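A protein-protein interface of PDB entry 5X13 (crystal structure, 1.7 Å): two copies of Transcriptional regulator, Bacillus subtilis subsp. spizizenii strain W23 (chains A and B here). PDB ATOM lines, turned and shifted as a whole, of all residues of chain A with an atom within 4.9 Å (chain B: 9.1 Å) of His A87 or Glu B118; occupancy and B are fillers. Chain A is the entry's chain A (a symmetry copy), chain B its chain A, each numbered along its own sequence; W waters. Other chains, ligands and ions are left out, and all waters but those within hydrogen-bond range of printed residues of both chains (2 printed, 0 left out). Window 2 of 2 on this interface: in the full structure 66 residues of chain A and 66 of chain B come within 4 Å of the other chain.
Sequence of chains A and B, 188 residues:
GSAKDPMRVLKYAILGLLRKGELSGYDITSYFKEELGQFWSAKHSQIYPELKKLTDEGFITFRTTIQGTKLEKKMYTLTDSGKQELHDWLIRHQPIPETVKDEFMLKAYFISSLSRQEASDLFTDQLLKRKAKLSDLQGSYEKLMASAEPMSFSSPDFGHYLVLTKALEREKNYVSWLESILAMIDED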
ATOM      1  N   LYS A  83     -21.980   6.766 -10.978  1.00  0.00           N
ATOM      2  CA  LYS A  83     -22.662   6.507  -9.708  1.00  0.00           C
ATOM      3  C   LYS A  83     -21.703   6.692  -8.535  1.00  0.00           C
ATOM      4  O   LYS A  83     -22.058   7.264  -7.492  1.00  0.00           O
ATOM      5  CB  LYS A  83     -23.251   5.107  -9.711  1.00  0.00           C
ATOM      6  CG  LYS A  83     -24.413   4.938 -10.642  1.00  0.00           C
ATOM      7  CD  LYS A  83     -25.082   3.589 -10.531  1.00  0.00           C
ATOM      8  CE  LYS A  83     -26.071   3.380 -11.682  1.00  0.00           C
ATOM      9  NZ  LYS A  83     -26.440   1.949 -11.837  1.00  0.00           N
ATOM     10  N   GLN A  84     -20.492   6.168  -8.695  1.00  0.00           N
ATOM     11  CA  GLN A  84     -19.444   6.312  -7.664  1.00  0.00           C
ATOM     12  C   GLN A  84     -19.032   7.800  -7.464  1.00  0.00           C
ATOM     13  O   GLN A  84     -18.889   8.282  -6.326  1.00  0.00           O
ATOM     14  CB  GLN A  84     -18.226   5.428  -7.989  1.00  0.00           C
ATOM     15  CG  GLN A  84     -17.259   5.339  -6.814  1.00  0.00           C
ATOM     16  CD  GLN A  84     -17.810   4.558  -5.616  1.00  0.00           C
ATOM     17  OE1 GLN A  84     -18.252   3.405  -5.764  1.00  0.00           O
ATOM     18  NE2 GLN A  84     -17.772   5.174  -4.406  1.00  0.00           N
ATOM     19  N   GLU A  85     -18.930   8.538  -8.562  1.00  0.00           N
ATOM     20  CA  GLU A  85     -18.520   9.944  -8.551  1.00  0.00           C
ATOM     21  C   GLU A  85     -19.581  10.751  -7.778  1.00  0.00           C
ATOM     22  O   GLU A  85     -19.259  11.551  -6.867  1.00  0.00           O
ATOM     23  CB  GLU A  85     -18.349  10.439  -9.991  1.00  0.00           C
ATOM     24  CG  GLU A  85     -17.666  11.808 -10.176  1.00  0.00           C
ATOM     25  CD  GLU A  85     -16.157  11.812  -9.918  1.00  0.00           C
ATOM     26  OE1 GLU A  85     -15.553  10.756  -9.508  1.00  0.00           O
ATOM     27  OE2 GLU A  85     -15.518  12.892 -10.108  1.00  0.00           O
ATOM     28  N   LEU A  86     -20.847  10.452  -8.067  1.00  0.00           N
ATOM     29  CA  LEU A  86     -21.980  11.077  -7.352  1.00  0.00           C
ATOM     30  C   LEU A  86     -21.982  10.731  -5.870  1.00  0.00           C
ATOM     31  O   LEU A  86     -22.103  11.595  -4.991  1.00  0.00           O
ATOM     32  CB  LEU A  86     -23.312  10.658  -7.997  1.00  0.00           C
ATOM     33  CG  LEU A  86     -24.596  11.164  -7.334  1.00  0.00           C
ATOM     34  CD1 LEU A  86     -24.662  12.685  -7.468  1.00  0.00           C
ATOM     35  CD2 LEU A  86     -25.810  10.444  -7.986  1.00  0.00           C
ATOM     36  N   HIS A  87     -21.816   9.442  -5.591  1.00  0.00           N
ATOM     37  CA  HIS A  87     -21.799   8.978  -4.236  1.00  0.00           C
ATOM     38  C   HIS A  87     -20.693   9.639  -3.420  1.00  0.00           C
ATOM     39  O   HIS A  87     -20.936  10.092  -2.275  1.00  0.00           O
ATOM     40  CB  HIS A  87     -21.649   7.454  -4.191  1.00  0.00           C
ATOM     41  CG  HIS A  87     -21.565   6.900  -2.801  1.00  0.00           C
ATOM     42  ND1 HIS A  87     -22.693   6.729  -2.020  1.00  0.00           N
ATOM     43  CD2 HIS A  87     -20.516   6.461  -2.053  1.00  0.00           C
ATOM     44  CE1 HIS A  87     -22.339   6.222  -0.847  1.00  0.00           C
ATOM     45  NE2 HIS A  87     -21.026   6.041  -0.844  1.00  0.00           N
ATOM     46  N   ASP A  88     -19.475   9.621  -3.955  1.00  0.00           N
ATOM     47  CA  ASP A  88     -18.338  10.176  -3.215  1.00  0.00           C
ATOM     48  C   ASP A  88     -18.579  11.669  -2.858  1.00  0.00           C
ATOM     49  O   ASP A  88     -18.201  12.133  -1.799  1.00  0.00           O
ATOM     50  CB  ASP A  88     -17.077  10.027  -4.064  1.00  0.00           C
ATOM     51  CG  ASP A  88     -16.567   8.561  -4.136  1.00  0.00           C
ATOM     52  OD1 ASP A  88     -17.045   7.705  -3.352  1.00  0.00           O
ATOM     53  OD2 ASP A  88     -15.727   8.295  -5.052  1.00  0.00           O
ATOM     54  N   TRP A  89     -19.169  12.405  -3.805  1.00  0.00           N
ATOM     55  CA  TRP A  89     -19.502  13.824  -3.592  1.00  0.00           C
ATOM     56  C   TRP A  89     -20.577  13.986  -2.527  1.00  0.00           C
ATOM     57  O   TRP A  89     -20.458  14.826  -1.646  1.00  0.00           O
ATOM     58  CB  TRP A  89     -19.985  14.422  -4.887  1.00  0.00           C
ATOM     59  CG  TRP A  89     -20.598  15.758  -4.825  1.00  0.00           C
ATOM     60  CD1 TRP A  89     -19.972  16.957  -4.724  1.00  0.00           C
ATOM     61  CD2 TRP A  89     -21.978  16.042  -5.003  1.00  0.00           C
ATOM     62  NE1 TRP A  89     -20.881  17.967  -4.771  1.00  0.00           N
ATOM     63  CE2 TRP A  89     -22.130  17.428  -4.924  1.00  0.00           C
ATOM     64  CE3 TRP A  89     -23.107  15.248  -5.178  1.00  0.00           C
ATOM     65  CZ2 TRP A  89     -23.386  18.051  -5.036  1.00  0.00           C
ATOM     66  CZ3 TRP A  89     -24.314  15.844  -5.294  1.00  0.00           C
ATOM     67  CH2 TRP A  89     -24.453  17.241  -5.241  1.00  0.00           C
ATOM     68  N   LEU A  90     -21.608  13.157  -2.596  1.00  0.00           N
ATOM     69  CA  LEU A  90     -22.715  13.212  -1.612  1.00  0.00           C
ATOM     70  C   LEU A  90     -22.198  13.013  -0.203  1.00  0.00           C
ATOM     71  O   LEU A  90     -22.602  13.726   0.725  1.00  0.00           O
ATOM     72  CB  LEU A  90     -23.813  12.173  -1.928  1.00  0.00           C
ATOM     73  CG  LEU A  90     -24.718  12.525  -3.098  1.00  0.00           C
ATOM     74  CD1 LEU A  90     -25.519  11.290  -3.468  1.00  0.00           C
ATOM     75  CD2 LEU A  90     -25.620  13.750  -2.769  1.00  0.00           C
ATOM     76  N   ILE A  91     -21.298  12.060  -0.023  1.00  0.00           N
ATOM     77  CA  ILE A  91     -20.855  11.781   1.345  1.00  0.00           C
ATOM     78  C   ILE A  91     -19.653  12.580   1.835  1.00  0.00           C
ATOM     79  O   ILE A  91     -19.362  12.551   3.066  1.00  0.00           O
ATOM     80  CB  ILE A  91     -20.671  10.280   1.577  1.00  0.00           C
ATOM     81  CG1 ILE A  91     -19.491   9.746   0.813  1.00  0.00           C
ATOM     82  CG2 ILE A  91     -22.012   9.543   1.276  1.00  0.00           C
ATOM     83  CD1 ILE A  91     -19.028   8.335   1.317  1.00  0.00           C
ATOM     84  N   PHE B 104     -24.568  22.067  -0.382  1.00  0.00           N
ATOM     85  CA  PHE B 104     -25.245  21.145   0.495  1.00  0.00           C
ATOM     86  C   PHE B 104     -26.667  20.884   0.040  1.00  0.00           C
ATOM     87  O   PHE B 104     -27.173  19.776   0.136  1.00  0.00           O
ATOM     88  CB  PHE B 104     -25.247  21.640   1.967  1.00  0.00           C
ATOM     89  CG  PHE B 104     -25.994  20.729   2.882  1.00  0.00           C
ATOM     90  CD1 PHE B 104     -25.432  19.583   3.390  1.00  0.00           C
ATOM     91  CD2 PHE B 104     -27.287  21.010   3.241  1.00  0.00           C
ATOM     92  CE1 PHE B 104     -26.158  18.741   4.204  1.00  0.00           C
ATOM     93  CE2 PHE B 104     -27.995  20.188   4.037  1.00  0.00           C
ATOM     94  CZ  PHE B 104     -27.442  19.055   4.532  1.00  0.00           C
ATOM     95  N   LYS B 107     -26.961  18.437  -2.728  1.00  0.00           N
ATOM     96  CA  LYS B 107     -26.881  17.101  -2.187  1.00  0.00           C
ATOM     97  C   LYS B 107     -28.229  16.675  -1.613  1.00  0.00           C
ATOM     98  O   LYS B 107     -28.718  15.564  -1.875  1.00  0.00           O
ATOM     99  CB  LYS B 107     -25.790  17.050  -1.109  1.00  0.00           C
ATOM    100  CG  LYS B 107     -24.395  17.272  -1.625  1.00  0.00           C
ATOM    101  CD  LYS B 107     -23.300  17.097  -0.556  1.00  0.00           C
ATOM    102  CE  LYS B 107     -21.997  17.506  -1.234  1.00  0.00           C
ATOM    103  NZ  LYS B 107     -20.732  17.368  -0.396  1.00  0.00           N
ATOM    104  N   PHE B 110     -30.696  15.445  -4.093  1.00  0.00           N
ATOM    105  CA  PHE B 110     -30.391  14.083  -4.552  1.00  0.00           C
ATOM    106  C   PHE B 110     -30.299  13.078  -3.433  1.00  0.00           C
ATOM    107  O   PHE B 110     -29.682  11.989  -3.553  1.00  0.00           O
ATOM    108  CB  PHE B 110     -29.069  14.161  -5.339  1.00  0.00           C
ATOM    109  CG  PHE B 110     -29.157  15.037  -6.582  1.00  0.00           C
ATOM    110  CD1 PHE B 110     -30.219  14.909  -7.494  1.00  0.00           C
ATOM    111  CD2 PHE B 110     -28.182  15.991  -6.849  1.00  0.00           C
ATOM    112  CE1 PHE B 110     -30.312  15.692  -8.626  1.00  0.00           C
ATOM    113  CE2 PHE B 110     -28.255  16.779  -8.018  1.00  0.00           C
ATOM    114  CZ  PHE B 110     -29.301  16.626  -8.910  1.00  0.00           C
ATOM    115  N   ILE B 111     -30.940  13.411  -2.315  1.00  0.00           N
ATOM    116  CA  ILE B 111     -30.930  12.523  -1.139  1.00  0.00           C
ATOM    117  C   ILE B 111     -31.412  11.079  -1.416  1.00  0.00           C
ATOM    118  O   ILE B 111     -31.026  10.135  -0.677  1.00  0.00           O
ATOM    119  CB  ILE B 111     -31.771  13.146   0.003  1.00  0.00           C
ATOM    120  CG1 ILE B 111     -31.405  12.496   1.355  1.00  0.00           C
ATOM    121  CG2 ILE B 111     -33.287  13.101  -0.330  1.00  0.00           C
ATOM    122  CD1 ILE B 111     -31.983  13.232   2.576  1.00  0.00           C
ATOM    123  N   SER B 112     -32.171  10.870  -2.484  1.00  0.00           N
ATOM    124  CA  SER B 112     -32.622   9.503  -2.795  1.00  0.00           C
ATOM    125  C   SER B 112     -31.443   8.519  -3.004  1.00  0.00           C
ATOM    126  O   SER B 112     -31.630   7.325  -2.870  1.00  0.00           O
ATOM    127  CB  SER B 112     -33.560   9.435  -3.985  1.00  0.00           C
ATOM    128  OG  SER B 112     -32.902   9.752  -5.215  1.00  0.00           O
ATOM    129  N   SER B 113     -30.276   9.049  -3.360  1.00  0.00           N
ATOM    130  CA  SER B 113     -29.079   8.232  -3.556  1.00  0.00           C
ATOM    131  C   SER B 113     -28.374   7.834  -2.284  1.00  0.00           C
ATOM    132  O   SER B 113     -27.360   7.126  -2.350  1.00  0.00           O
ATOM    133  CB  SER B 113     -28.104   8.973  -4.469  1.00  0.00           C
ATOM    134  OG  SER B 113     -28.613   9.004  -5.797  1.00  0.00           O
ATOM    135  N   LEU B 114     -28.927   8.241  -1.124  1.00  0.00           N
ATOM    136  CA  LEU B 114     -28.385   7.900   0.195  1.00  0.00           C
ATOM    137  C   LEU B 114     -29.345   7.040   1.000  1.00  0.00           C
ATOM    138  O   LEU B 114     -30.559   7.234   0.988  1.00  0.00           O
ATOM    139  CB  LEU B 114     -28.087   9.167   0.999  1.00  0.00           C
ATOM    140  CG  LEU B 114     -27.021  10.093   0.354  1.00  0.00           C
ATOM    141  CD1 LEU B 114     -26.744  11.348   1.200  1.00  0.00           C
ATOM    142  CD2 LEU B 114     -25.725   9.373   0.095  1.00  0.00           C
ATOM    143  N   SER B 115     -28.772   6.117   1.796  1.00  0.00           N
ATOM    144  CA  SER B 115     -29.556   5.381   2.736  1.00  0.00           C
ATOM    145  C   SER B 115     -30.004   6.313   3.884  1.00  0.00           C
ATOM    146  O   SER B 115     -29.502   7.410   4.041  1.00  0.00           O
ATOM    147  CB  SER B 115     -28.732   4.233   3.316  1.00  0.00           C
ATOM    148  OG  SER B 115     -27.770   4.733   4.226  1.00  0.00           O
ATOM    149  N   ARG B 116     -30.941   5.839   4.682  1.00  0.00           N
ATOM    150  CA  ARG B 116     -31.400   6.598   5.861  1.00  0.00           C
ATOM    151  C   ARG B 116     -30.216   6.966   6.741  1.00  0.00           C
ATOM    152  O   ARG B 116     -30.086   8.114   7.185  1.00  0.00           O
ATOM    153  CB  ARG B 116     -32.488   5.821   6.622  1.00  0.00           C
ATOM    154  CG  ARG B 116     -33.239   6.673   7.644  1.00  0.00           C
ATOM    155  CD  ARG B 116     -34.241   5.897   8.472  1.00  0.00           C
ATOM    156  NE  ARG B 116     -35.357   5.343   7.681  1.00  0.00           N
ATOM    157  CZ  ARG B 116     -36.507   5.950   7.376  1.00  0.00           C
ATOM    158  NH1 ARG B 116     -36.787   7.182   7.776  1.00  0.00           N
ATOM    159  NH2 ARG B 116     -37.412   5.290   6.645  1.00  0.00           N
ATOM    160  N   GLN B 117     -29.334   6.006   7.019  1.00  0.00           N
ATOM    161  CA  GLN B 117     -28.188   6.325   7.856  1.00  0.00           C
ATOM    162  C   GLN B 117     -27.233   7.305   7.195  1.00  0.00           C
ATOM    163  O   GLN B 117     -26.745   8.229   7.850  1.00  0.00           O
ATOM    164  CB  GLN B 117     -27.444   5.077   8.328  1.00  0.00           C
ATOM    165  CG  GLN B 117     -26.364   5.417   9.366  1.00  0.00           C
ATOM    166  CD  GLN B 117     -26.916   6.089  10.650  1.00  0.00           C
ATOM    167  OE1 GLN B 117     -27.914   5.616  11.258  1.00  0.00           O
ATOM    168  NE2 GLN B 117     -26.301   7.207  11.041  1.00  0.00           N
ATOM    169  N   GLU B 118     -26.981   7.132   5.893  1.00  0.00           N
ATOM    170  CA  GLU B 118     -26.089   8.073   5.193  1.00  0.00           C
ATOM    171  C   GLU B 118     -26.690   9.480   5.179  1.00  0.00           C
ATOM    172  O   GLU B 118     -25.946  10.468   5.341  1.00  0.00           O
ATOM    173  CB  GLU B 118     -25.763   7.623   3.775  1.00  0.00           C
ATOM    174  CG  GLU B 118     -24.920   6.390   3.674  1.00  0.00           C
ATOM    175  CD  GLU B 118     -24.886   5.805   2.262  1.00  0.00           C
ATOM    176  OE1 GLU B 118     -25.927   5.845   1.563  1.00  0.00           O
ATOM    177  OE2 GLU B 118     -23.823   5.272   1.874  1.00  0.00           O
ATOM    178  N   ALA B 119     -28.008   9.571   5.027  1.00  0.00           N
ATOM    179  CA  ALA B 119     -28.681  10.876   5.029  1.00  0.00           C
ATOM    180  C   ALA B 119     -28.569  11.507   6.425  1.00  0.00           C
ATOM    181  O   ALA B 119     -28.269  12.697   6.576  1.00  0.00           O
ATOM    182  CB  ALA B 119     -30.158  10.732   4.551  1.00  0.00           C
ATOM    183  N   SER B 120     -28.771  10.691   7.450  1.00  0.00           N
ATOM    184  CA  SER B 120     -28.677  11.194   8.800  1.00  0.00           C
ATOM    185  C   SER B 120     -27.239  11.695   9.024  1.00  0.00           C
ATOM    186  O   SER B 120     -27.017  12.730   9.619  1.00  0.00           O
ATOM    187  CB  SER B 120     -29.023  10.071   9.770  1.00  0.00           C
ATOM    188  OG  SER B 120     -28.906  10.532  11.096  1.00  0.00           O
ATOM    189  N   ASP B 121     -26.246  10.959   8.539  1.00  0.00           N
ATOM    190  CA  ASP B 121     -24.861  11.368   8.788  1.00  0.00           C
ATOM    191  C   ASP B 121     -24.522  12.678   8.046  1.00  0.00           C
ATOM    192  O   ASP B 121     -23.797  13.541   8.586  1.00  0.00           O
ATOM    193  CB  ASP B 121     -23.908  10.221   8.457  1.00  0.00           C
ATOM    194  CG  ASP B 121     -24.006   9.045   9.454  1.00  0.00           C
ATOM    195  OD1 ASP B 121     -24.574   9.144  10.556  1.00  0.00           O
ATOM    196  OD2 ASP B 121     -23.474   7.977   9.116  1.00  0.00           O
ATOM    197  N   LEU B 122     -24.992  12.795   6.823  1.00  0.00           N
ATOM    198  CA  LEU B 122     -24.811  14.027   6.017  1.00  0.00           C
ATOM    199  C   LEU B 122     -25.415  15.255   6.691  1.00  0.00           C
ATOM    200  O   LEU B 122     -24.764  16.286   6.858  1.00  0.00           O
ATOM    201  CB  LEU B 122     -25.396  13.839   4.643  1.00  0.00           C
ATOM    202  CG  LEU B 122     -25.413  15.106   3.764  1.00  0.00           C
ATOM    203  CD1 LEU B 122     -23.997  15.557   3.480  1.00  0.00           C
ATOM    204  CD2 LEU B 122     -26.281  14.914   2.505  1.00  0.00           C
ATOM    205  N   PHE B 123     -26.654  15.111   7.140  1.00  0.00           N
ATOM    206  CA  PHE B 123     -27.364  16.227   7.767  1.00  0.00           C
ATOM    207  C   PHE B 123     -26.820  16.548   9.175  1.00  0.00           C
ATOM    208  O   PHE B 123     -26.782  17.723   9.532  1.00  0.00           O
ATOM    209  CB  PHE B 123     -28.875  15.938   7.820  1.00  0.00           C
ATOM    210  CG  PHE B 123     -29.587  16.379   6.598  1.00  0.00           C
ATOM    211  CD1 PHE B 123     -29.368  15.735   5.407  1.00  0.00           C
ATOM    212  CD2 PHE B 123     -30.392  17.496   6.635  1.00  0.00           C
ATOM    213  CE1 PHE B 123     -30.022  16.212   4.244  1.00  0.00           C
ATOM    214  CE2 PHE B 123     -30.981  17.944   5.510  1.00  0.00           C
ATOM    215  CZ  PHE B 123     -30.765  17.283   4.321  1.00  0.00           C
ATOM    216  N   THR B 124     -26.371  15.528   9.906  1.00  0.00           N
ATOM    217  CA  THR B 124     -25.774  15.699  11.241  1.00  0.00           C
ATOM    218  C   THR B 124     -24.482  16.469  11.102  1.00  0.00           C
ATOM    219  O   THR B 124     -24.222  17.368  11.863  1.00  0.00           O
ATOM    220  CB  THR B 124     -25.561  14.362  11.958  1.00  0.00           C
ATOM    221  OG1 THR B 124     -26.826  13.710  12.157  1.00  0.00           O
ATOM    222  CG2 THR B 124     -24.923  14.565  13.322  1.00  0.00           C
ATOM    223  N   ASP B 125     -23.672  16.133  10.094  1.00  0.00           N
ATOM    224  CA  ASP B 125     -22.388  16.847   9.888  1.00  0.00           C
ATOM    225  C   ASP B 125     -22.670  18.345   9.628  1.00  0.00           C
ATOM    226  O   ASP B 125     -22.027  19.238  10.217  1.00  0.00           O
ATOM    227  CB  ASP B 125     -21.663  16.227   8.706  1.00  0.00           C
ATOM    228  CG  ASP B 125     -20.357  16.994   8.347  1.00  0.00           C
ATOM    229  OD1 ASP B 125     -19.357  16.828   9.090  1.00  0.00           O
ATOM    230  OD2 ASP B 125     -20.393  17.746   7.390  1.00  0.00           O
ATOM    231  N   LEU B 182     -33.671  16.176  10.226  1.00  0.00           N
ATOM    232  CA  LEU B 182     -33.123  15.041  10.938  1.00  0.00           C
ATOM    233  C   LEU B 182     -34.263  14.318  11.676  1.00  0.00           C
ATOM    234  O   LEU B 182     -34.274  13.100  11.734  1.00  0.00           O
ATOM    235  CB  LEU B 182     -32.093  15.497  11.918  1.00  0.00           C
ATOM    236  CG  LEU B 182     -30.708  15.811  11.287  1.00  0.00           C
ATOM    237  CD1 LEU B 182     -29.873  16.623  12.269  1.00  0.00           C
ATOM    238  CD2 LEU B 182     -30.005  14.462  10.883  1.00  0.00           C
ATOM    239  N   ILE B 185     -35.896  12.209   9.022  1.00  0.00           N
ATOM    240  CA  ILE B 185     -35.032  11.087   8.691  1.00  0.00           C
ATOM    241  C   ILE B 185     -35.208  10.033   9.822  1.00  0.00           C
ATOM    242  O   ILE B 185     -35.351   8.828   9.526  1.00  0.00           O
ATOM    243  CB  ILE B 185     -33.576  11.547   8.498  1.00  0.00           C
ATOM    244  CG1 ILE B 185     -33.456  12.373   7.197  1.00  0.00           C
ATOM    245  CG2 ILE B 185     -32.602  10.389   8.369  1.00  0.00           C
ATOM    246  CD1 ILE B 185     -32.180  13.176   7.162  1.00  0.00           C
HETATM  247  O   HOH W   1     -24.851   7.426  -3.572  1.00  0.00           O
HETATM  248  O   HOH W   2     -25.647   5.481  -1.031  1.00  0.00           O
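The backbone carbonyl oxygen (O) of Trp A89 sits at hydrogen-bond distance from the side-chain amino group (NZ) of Lys B107.
The side-chain carboxylate of Glu B118 lies within hydrogen-bond range of the backbone NH of Ser B115 (2.9 Å).
Among the printed residues, merely in contact across the chains: Leu A86 with Ser B113 (3.8 Å), His A87 with Glu B118 (3.2 Å), Leu A90 with Lys B107 (3.6 Å), Leu A90 with Ser B113 (3.6 Å), Leu A90 with Leu B114 (3.9 Å), Leu A90 with Leu B122 (3.6 Å) and Ile A91 with Leu B114 (3.9 Å).
Printed residues of chain B within 4 Å of Ile A91: Leu B114 (3.9 Å). Ser B112 touches none of the printed residues of chain A. Printed residues of chain A within 4 Å of Ser B113: Leu A86 and Leu A90. Of the printed residues of chain A, Leu B114 touches Leu A90 (3.9 Å) and Ile A91 (3.9 Å). Arg B116 touches none of the printed residues of chain A. Glu B118 touches just one residue of chain A: His A87 (3.2 Å). The nearest residue of chain B that does not touch His A87 is Leu B114 (4.5 Å). The nearest printed residue of chain A that does not touch Ser B113 is His A87 (4.7 Å).
Printed residues of chain B that touch a printed residue of chain A: Lys B107, Ser B113, Leu B114, Glu B118 and Leu B122. Along chain B the printed residues that touch a printed residue of chain A span positions 107 to 122. Of the 9 printed residues of chain A, 5 touch a printed residue of chain B. Among the printed residues, 8 pairs touch across the chains. Among the printed residues, no Asp or Glu carboxylate lies within 4 Å of a Lys or Arg side-chain nitrogen of the other chain.
No position is printed for both chains. Of the 8 pairs that touch across the chains among the printed residues, none has its exchanged pair printed and touching as well.
Water W2 lies within hydrogen-bond range of OE1 of Glu B118 (2.6 Å), O of Ser B113 (2.7 Å) and ND1 of His A87 (3.4 Å). Water W1 bridges a ring nitrogen (ND1) of His A87 (2.7 Å) and the backbone carbonyl oxygen (O) of Ser B113 (2.8 Å).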
